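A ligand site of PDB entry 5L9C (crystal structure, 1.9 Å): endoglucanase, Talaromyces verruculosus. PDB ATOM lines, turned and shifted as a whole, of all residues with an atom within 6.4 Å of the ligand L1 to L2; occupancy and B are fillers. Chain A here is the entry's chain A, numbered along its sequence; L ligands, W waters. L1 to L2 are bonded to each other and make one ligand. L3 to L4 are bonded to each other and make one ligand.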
ATOM      1  N   HIS A 102      17.477 -23.897  -5.176  1.00  0.00           N
ATOM      2  CA  HIS A 102      18.633 -24.755  -5.426  1.00  0.00           C
ATOM      3  C   HIS A 102      19.075 -24.618  -6.886  1.00  0.00           C
ATOM      4  O   HIS A 102      18.999 -25.546  -7.693  1.00  0.00           O
ATOM      5  CB  HIS A 102      18.270 -26.203  -5.094  1.00  0.00           C
ATOM      6  CG  HIS A 102      19.396 -27.005  -4.514  1.00  0.00           C
ATOM      7  ND1 HIS A 102      19.832 -26.840  -3.212  1.00  0.00           N
ATOM      8  CD2 HIS A 102      20.157 -27.980  -5.050  1.00  0.00           C
ATOM      9  CE1 HIS A 102      20.809 -27.694  -2.976  1.00  0.00           C
ATOM     10  NE2 HIS A 102      21.038 -28.385  -4.069  1.00  0.00           N
ATOM     11  N   PHE A 104      22.108 -22.538  -8.106  1.00  0.00           N
ATOM     12  CA  PHE A 104      23.518 -22.309  -8.457  1.00  0.00           C
ATOM     13  C   PHE A 104      23.731 -20.945  -9.126  1.00  0.00           C
ATOM     14  O   PHE A 104      24.642 -20.777  -9.948  1.00  0.00           O
ATOM     15  CB  PHE A 104      24.063 -23.428  -9.339  1.00  0.00           C
ATOM     16  CG  PHE A 104      23.916 -24.803  -8.725  1.00  0.00           C
ATOM     17  CD1 PHE A 104      22.774 -25.550  -8.946  1.00  0.00           C
ATOM     18  CD2 PHE A 104      24.909 -25.321  -7.911  1.00  0.00           C
ATOM     19  CE1 PHE A 104      22.616 -26.802  -8.367  1.00  0.00           C
ATOM     20  CE2 PHE A 104      24.765 -26.574  -7.335  1.00  0.00           C
ATOM     21  CZ  PHE A 104      23.622 -27.313  -7.561  1.00  0.00           C
ATOM     22  N   ASN A 141      21.467 -21.499  -3.664  1.00  0.00           N
ATOM     23  CA  ASN A 141      22.376 -22.586  -3.351  1.00  0.00           C
ATOM     24  C   ASN A 141      23.578 -22.531  -4.291  1.00  0.00           C
ATOM     25  O   ASN A 141      23.428 -22.752  -5.498  1.00  0.00           O
ATOM     26  CB  ASN A 141      21.672 -23.931  -3.468  1.00  0.00           C
ATOM     27  CG  ASN A 141      22.642 -25.103  -3.363  1.00  0.00           C
ATOM     28  OD1 ASN A 141      23.254 -25.317  -2.328  1.00  0.00           O
ATOM     29  ND2 ASN A 141      22.771 -25.872  -4.450  1.00  0.00           N
ATOM     30  N   GLU A 142      24.755 -22.227  -3.748  1.00  0.00           N
ATOM     31  CA  GLU A 142      26.043 -22.441  -4.403  1.00  0.00           C
ATOM     32  C   GLU A 142      26.149 -21.674  -5.728  1.00  0.00           C
ATOM     33  O   GLU A 142      26.162 -22.245  -6.820  1.00  0.00           O
ATOM     34  CB  GLU A 142      26.308 -23.939  -4.617  1.00  0.00           C
ATOM     35  CG  GLU A 142      26.262 -24.753  -3.329  1.00  0.00           C
ATOM     36  CD  GLU A 142      26.748 -26.186  -3.494  1.00  0.00           C
ATOM     37  OE1 GLU A 142      26.887 -26.646  -4.652  1.00  0.00           O
ATOM     38  OE2 GLU A 142      26.989 -26.858  -2.469  1.00  0.00           O
ATOM     39  N   ALA A 178      32.011 -19.757  -5.813  1.00  0.00           N
ATOM     40  CA  ALA A 178      32.820 -20.979  -5.724  1.00  0.00           C
ATOM     41  C   ALA A 178      32.122 -22.057  -4.898  1.00  0.00           C
ATOM     42  O   ALA A 178      32.740 -22.733  -4.072  1.00  0.00           O
ATOM     43  CB  ALA A 178      34.208 -20.675  -5.152  1.00  0.00           C
ATOM     44  N   TYR A 179      30.816 -22.222  -5.135  1.00  0.00           N
ATOM     45  CA  TYR A 179      29.966 -23.194  -4.436  1.00  0.00           C
ATOM     46  C   TYR A 179      29.933 -22.953  -2.927  1.00  0.00           C
ATOM     47  O   TYR A 179      29.639 -23.885  -2.167  1.00  0.00           O
ATOM     48  CB  TYR A 179      30.413 -24.640  -4.735  1.00  0.00           C
ATOM     49  CG  TYR A 179      30.461 -24.988  -6.205  1.00  0.00           C
ATOM     50  CD1 TYR A 179      29.344 -25.488  -6.855  1.00  0.00           C
ATOM     51  CD2 TYR A 179      31.631 -24.826  -6.944  1.00  0.00           C
ATOM     52  CE1 TYR A 179      29.378 -25.823  -8.203  1.00  0.00           C
ATOM     53  CE2 TYR A 179      31.681 -25.145  -8.291  1.00  0.00           C
ATOM     54  CZ  TYR A 179      30.550 -25.647  -8.907  1.00  0.00           C
ATOM     55  OH  TYR A 179      30.600 -25.967 -10.254  1.00  0.00           O
ATOM     56  N   GLY A 181      32.099 -22.809  -0.737  1.00  0.00           N
ATOM     57  CA  GLY A 181      32.910 -23.757   0.018  1.00  0.00           C
ATOM     58  C   GLY A 181      33.639 -23.076   1.164  1.00  0.00           C
ATOM     59  O   GLY A 181      34.105 -21.952   1.055  1.00  0.00           O
ATOM     60  N   TRP A 183      36.488 -24.154   2.572  1.00  0.00           N
ATOM     61  CA  TRP A 183      37.918 -24.250   2.368  1.00  0.00           C
ATOM     62  C   TRP A 183      38.487 -23.192   1.461  1.00  0.00           C
ATOM     63  O   TRP A 183      39.665 -22.945   1.519  1.00  0.00           O
ATOM     64  CB  TRP A 183      38.333 -25.641   1.911  1.00  0.00           C
ATOM     65  CG  TRP A 183      37.747 -26.153   0.659  1.00  0.00           C
ATOM     66  CD1 TRP A 183      36.447 -26.300   0.344  1.00  0.00           C
ATOM     67  CD2 TRP A 183      38.484 -26.720  -0.422  1.00  0.00           C
ATOM     68  NE1 TRP A 183      36.314 -26.896  -0.869  1.00  0.00           N
ATOM     69  CE2 TRP A 183      37.561 -27.158  -1.365  1.00  0.00           C
ATOM     70  CE3 TRP A 183      39.844 -26.898  -0.679  1.00  0.00           C
ATOM     71  CZ2 TRP A 183      37.957 -27.747  -2.557  1.00  0.00           C
ATOM     72  CZ3 TRP A 183      40.223 -27.459  -1.832  1.00  0.00           C
ATOM     73  CH2 TRP A 183      39.293 -27.877  -2.780  1.00  0.00           C
ATOM     74  N   THR A 184      37.661 -22.653   0.572  1.00  0.00           N
ATOM     75  CA  THR A 184      38.072 -21.633  -0.371  1.00  0.00           C
ATOM     76  C   THR A 184      37.494 -20.266  -0.047  1.00  0.00           C
ATOM     77  O   THR A 184      37.602 -19.349  -0.877  1.00  0.00           O
ATOM     78  CB  THR A 184      37.688 -22.035  -1.800  1.00  0.00           C
ATOM     79  OG1 THR A 184      36.263 -22.231  -1.879  1.00  0.00           O
ATOM     80  CG2 THR A 184      38.393 -23.329  -2.207  1.00  0.00           C
ATOM     81  N   HIS A 207      29.536 -24.663   2.701  1.00  0.00           N
ATOM     82  CA  HIS A 207      29.419 -26.097   2.514  1.00  0.00           C
ATOM     83  C   HIS A 207      30.809 -26.703   2.551  1.00  0.00           C
ATOM     84  O   HIS A 207      31.788 -26.081   2.141  1.00  0.00           O
ATOM     85  CB  HIS A 207      28.722 -26.426   1.185  1.00  0.00           C
ATOM     86  CG  HIS A 207      27.334 -25.860   1.077  1.00  0.00           C
ATOM     87  ND1 HIS A 207      26.621 -25.867  -0.098  1.00  0.00           N
ATOM     88  CD2 HIS A 207      26.531 -25.292   1.995  1.00  0.00           C
ATOM     89  CE1 HIS A 207      25.439 -25.312   0.096  1.00  0.00           C
ATOM     90  NE2 HIS A 207      25.353 -24.955   1.362  1.00  0.00           N
ATOM     91  N   GLN A 208      30.915 -27.929   3.069  1.00  0.00           N
ATOM     92  CA  GLN A 208      32.218 -28.569   3.121  1.00  0.00           C
ATOM     93  C   GLN A 208      32.081 -30.071   2.963  1.00  0.00           C
ATOM     94  O   GLN A 208      31.415 -30.726   3.770  1.00  0.00           O
ATOM     95  CB  GLN A 208      32.960 -28.232   4.421  1.00  0.00           C
ATOM     96  CG  GLN A 208      34.452 -28.530   4.343  1.00  0.00           C
ATOM     97  CD  GLN A 208      35.103 -27.853   3.142  1.00  0.00           C
ATOM     98  OE1 GLN A 208      35.201 -26.629   3.075  1.00  0.00           O
ATOM     99  NE2 GLN A 208      35.555 -28.656   2.177  1.00  0.00           N
ATOM    100  N   TYR A 209      32.708 -30.599   1.931  1.00  0.00           N
ATOM    101  CA  TYR A 209      32.872 -32.036   1.727  1.00  0.00           C
ATOM    102  C   TYR A 209      34.350 -32.389   1.830  1.00  0.00           C
ATOM    103  O   TYR A 209      35.224 -31.527   1.760  1.00  0.00           O
ATOM    104  CB  TYR A 209      32.293 -32.457   0.378  1.00  0.00           C
ATOM    105  CG  TYR A 209      30.792 -32.244   0.323  1.00  0.00           C
ATOM    106  CD1 TYR A 209      29.918 -33.208   0.814  1.00  0.00           C
ATOM    107  CD2 TYR A 209      30.259 -31.066  -0.196  1.00  0.00           C
ATOM    108  CE1 TYR A 209      28.549 -33.014   0.771  1.00  0.00           C
ATOM    109  CE2 TYR A 209      28.890 -30.872  -0.239  1.00  0.00           C
ATOM    110  CZ  TYR A 209      28.044 -31.846   0.251  1.00  0.00           C
ATOM    111  OH  TYR A 209      26.689 -31.653   0.205  1.00  0.00           O
ATOM    112  N   ASP A 213      38.366 -33.258  -4.178  1.00  0.00           N
ATOM    113  CA  ASP A 213      37.992 -32.010  -4.824  1.00  0.00           C
ATOM    114  C   ASP A 213      36.912 -31.241  -4.076  1.00  0.00           C
ATOM    115  O   ASP A 213      36.501 -30.169  -4.533  1.00  0.00           O
ATOM    116  CB  ASP A 213      37.536 -32.280  -6.268  1.00  0.00           C
ATOM    117  CG  ASP A 213      36.346 -33.212  -6.345  1.00  0.00           C
ATOM    118  OD1 ASP A 213      35.755 -33.550  -5.298  1.00  0.00           O
ATOM    119  OD2 ASP A 213      35.985 -33.590  -7.490  1.00  0.00           O
ATOM    120  N   GLY A 214      36.441 -31.759  -2.948  1.00  0.00           N
ATOM    121  CA  GLY A 214      35.345 -31.110  -2.260  1.00  0.00           C
ATOM    122  C   GLY A 214      34.020 -31.144  -2.979  1.00  0.00           C
ATOM    123  O   GLY A 214      33.129 -30.358  -2.654  1.00  0.00           O
ATOM    124  N   SER A 215      33.856 -32.042  -3.956  1.00  0.00           N
ATOM    125  CA  SER A 215      32.599 -32.123  -4.679  1.00  0.00           C
ATOM    126  C   SER A 215      31.528 -32.854  -3.897  1.00  0.00           C
ATOM    127  O   SER A 215      30.339 -32.635  -4.147  1.00  0.00           O
ATOM    128  CB  SER A 215      32.806 -32.824  -6.022  1.00  0.00           C
ATOM    129  OG  SER A 215      33.247 -34.161  -5.846  1.00  0.00           O
ATOM    130  N   GLY A 216      31.910 -33.720  -2.949  1.00  0.00           N
ATOM    131  CA  GLY A 216      30.947 -34.519  -2.238  1.00  0.00           C
ATOM    132  C   GLY A 216      30.273 -35.501  -3.156  1.00  0.00           C
ATOM    133  O   GLY A 216      29.039 -35.615  -3.161  1.00  0.00           O
ATOM    134  N   THR A 217      31.069 -36.207  -3.958  1.00  0.00           N
ATOM    135  CA  THR A 217      30.544 -37.241  -4.844  1.00  0.00           C
ATOM    136  C   THR A 217      31.204 -38.594  -4.594  1.00  0.00           C
ATOM    137  O   THR A 217      30.943 -39.542  -5.340  1.00  0.00           O
ATOM    138  CB  THR A 217      30.724 -36.833  -6.312  1.00  0.00           C
ATOM    139  OG1 THR A 217      32.115 -36.658  -6.598  1.00  0.00           O
ATOM    140  CG2 THR A 217      29.980 -35.533  -6.589  1.00  0.00           C
ATOM    141  N   GLU A 249      25.805 -27.585   4.305  1.00  0.00           N
ATOM    142  CA  GLU A 249      25.960 -28.902   3.704  1.00  0.00           C
ATOM    143  C   GLU A 249      27.269 -29.522   4.157  1.00  0.00           C
ATOM    144  O   GLU A 249      28.322 -28.862   4.115  1.00  0.00           O
ATOM    145  CB  GLU A 249      25.933 -28.857   2.170  1.00  0.00           C
ATOM    146  CG  GLU A 249      24.621 -28.402   1.542  1.00  0.00           C
ATOM    147  CD  GLU A 249      24.636 -28.511   0.029  1.00  0.00           C
ATOM    148  OE1 GLU A 249      25.561 -29.159  -0.520  1.00  0.00           O
ATOM    149  OE2 GLU A 249      23.730 -27.938  -0.617  1.00  0.00           O
HETATM  150  C1  LIG L   1      34.771 -27.422  -5.916  1.00  0.00           C
HETATM  151  C2  LIG L   1      33.620 -28.412  -5.924  1.00  0.00           C
HETATM  152  C3  LIG L   1      32.909 -28.425  -7.277  1.00  0.00           C
HETATM  153  C4  LIG L   1      33.912 -28.552  -8.413  1.00  0.00           C
HETATM  154  C5  LIG L   1      33.214 -28.480  -9.770  1.00  0.00           C
HETATM  155  C6  LIG L   1      35.667 -27.613  -7.145  1.00  0.00           C
HETATM  156  O1  LIG L   1      36.686 -26.605  -7.149  1.00  0.00           O
HETATM  157  O2  LIG L   1      35.553 -27.604  -4.720  1.00  0.00           O
HETATM  158  O3  LIG L   1      32.683 -28.064  -4.901  1.00  0.00           O
HETATM  159  O4  LIG L   1      31.995 -29.513  -7.327  1.00  0.00           O
HETATM  160  O5  LIG L   1      34.883 -27.504  -8.323  1.00  0.00           O
HETATM  161  O6  LIG L   1      33.993 -29.179 -10.746  1.00  0.00           O
HETATM  162  C1  LG2 L   2      29.628 -29.837  -7.650  1.00  0.00           C
HETATM  163  C2  LG2 L   2      28.246 -29.542  -7.092  1.00  0.00           C
HETATM  164  C3  LG2 L   2      28.200 -29.783  -5.580  1.00  0.00           C
HETATM  165  C4  LG2 L   2      29.371 -29.089  -4.892  1.00  0.00           C
HETATM  166  C5  LG2 L   2      29.367 -29.388  -3.394  1.00  0.00           C
HETATM  167  C6  LG2 L   2      30.706 -29.145  -6.833  1.00  0.00           C
HETATM  168  O1  LG2 L   2      29.697 -29.389  -9.016  1.00  0.00           O
HETATM  169  O2  LG2 L   2      27.277 -30.381  -7.730  1.00  0.00           O
HETATM  170  O3  LG2 L   2      26.964 -29.291  -5.059  1.00  0.00           O
HETATM  171  O4  LG2 L   2      30.599 -29.533  -5.465  1.00  0.00           O
HETATM  172  O5  LG2 L   2      30.213 -28.460  -2.723  1.00  0.00           O
HETATM  173  C1  LG3 L   3      23.807 -35.424  -6.054  1.00  0.00           C
HETATM  174  C2  LG3 L   3      22.954 -35.574  -7.308  1.00  0.00           C
HETATM  175  C3  LG3 L   3      21.545 -35.049  -7.079  1.00  0.00           C
HETATM  176  C4  LG3 L   3      21.561 -33.662  -6.454  1.00  0.00           C
HETATM  177  C5  LG3 L   3      20.158 -33.172  -6.155  1.00  0.00           C
HETATM  178  C6  LG3 L   3      23.697 -34.013  -5.483  1.00  0.00           C
HETATM  179  O1  LG3 L   3      24.428 -33.931  -4.260  1.00  0.00           O
HETATM  180  O2  LG3 L   3      25.175 -35.702  -6.365  1.00  0.00           O
HETATM  181  O3  LG3 L   3      22.901 -36.954  -7.682  1.00  0.00           O
HETATM  182  O4  LG3 L   3      20.850 -34.994  -8.324  1.00  0.00           O
HETATM  183  O5  LG3 L   3      22.323 -33.699  -5.242  1.00  0.00           O
HETATM  184  O6  LG3 L   3      20.215 -32.040  -5.287  1.00  0.00           O
HETATM  185  C1  LG4 L   4      18.863 -35.581  -9.560  1.00  0.00           C
HETATM  186  C2  LG4 L   4      17.723 -36.588  -9.677  1.00  0.00           C
HETATM  187  C3  LG4 L   4      18.234 -38.019  -9.570  1.00  0.00           C
HETATM  188  C4  LG4 L   4      19.145 -38.182  -8.361  1.00  0.00           C
HETATM  189  C5  LG4 L   4      19.722 -39.586  -8.293  1.00  0.00           C
HETATM  190  C6  LG4 L   4      19.740 -35.893  -8.348  1.00  0.00           C
HETATM  191  O1  LG4 L   4      18.329 -34.269  -9.436  1.00  0.00           O
HETATM  192  O2  LG4 L   4      17.056 -36.409 -10.942  1.00  0.00           O
HETATM  193  O3  LG4 L   4      17.127 -38.914  -9.453  1.00  0.00           O
HETATM  194  O4  LG4 L   4      20.213 -37.237  -8.441  1.00  0.00           O
HETATM  195  O5  LG4 L   4      20.697 -39.665  -7.249  1.00  0.00           O
HETATM  196  O   HOH W   1      27.866 -33.153  -5.184  1.00  0.00           O
HETATM  197  O   HOH W   2      33.757 -26.242  -2.652  1.00  0.00           O
HETATM  198  O   HOH W   3      33.164 -29.981 -13.171  1.00  0.00           O
HETATM  199  O   HOH W   4      36.353 -24.119  -6.302  1.00  0.00           O
HETATM  200  O   HOH W   5      35.256 -26.093 -10.375  1.00  0.00           O
HETATM  201  O   HOH W   6      31.454 -26.222  -1.590  1.00  0.00           O
HETATM  202  O   HOH W   7      39.941 -27.167  -6.421  1.00  0.00           O
HETATM  203  O   HOH W   8      25.099 -30.780  -6.662  1.00  0.00           O
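Water W6 lies within hydrogen-bond range of an oxygen (O5) of LG2 L2 (2.8 Å) and the backbone carbonyl oxygen (O) of Tyr 179 (3.0 Å).
Water W2 bridges an oxygen (O2) of LIG L1 (3.1 Å) and the indole nitrogen (NE1) of Trp 183 (3.2 Å).
The side-chain carboxylate of Glu 142 is in hydrogen-bond range of a ring nitrogen (ND1) of His 207 (2.6 Å).
The side-chain hydroxyl (OG) of Ser 215 is in hydrogen-bond range of the side-chain carboxylate (OD1) of Asp 213, at 2.6 Å.
The side-chain amide oxygen (OE1) of Gln 208 lies within hydrogen-bond range of the backbone NH (N) of Trp 183 (2.8 Å).
OG of Ser 215 is in hydrogen-bond range of OG1 of Thr 217.
The side-chain hydroxyl (OH) of Tyr 209 lies within hydrogen-bond range of the side-chain carboxylate (OE1) of Glu 249, at 2.8 Å.
O of Ser 215 lies close to O4 of LG2 L2 (3.4 Å).
Merely in contact with the ligand L1 to L2: Tyr 179 (3.6 Å), Trp 183 (3.2 Å) and Tyr 209 (3.5 Å).
Hydrophobic or aromatic side chains within 4 Å of the ligand L1 to L2: Tyr 179, Trp 183 and Tyr 209.
Seven residues have an atom within 4 Å of the ligand L1 to L2: Glu 142, Tyr 179, Trp 183, Tyr 209, Asp 213, Gly 214 and Ser 215.
The nearest printed residue that does not touch the ligand L1 to L2 is Phe 104 (4.2 Å).
The side-chain carboxylate (OE1) of Glu 142 sits at hydrogen-bond distance from an oxygen (O3) of LG2 L2, at 2.7 Å.
The backbone carbonyl oxygen (O) of Asp 213 is in hydrogen-bond range of an oxygen (O2) of LIG L1, at 2.7 Å.
The backbone carbonyl oxygen (O) of Gly 214 lies within hydrogen-bond range of an oxygen (O3) of LIG L1 (3.2 Å).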
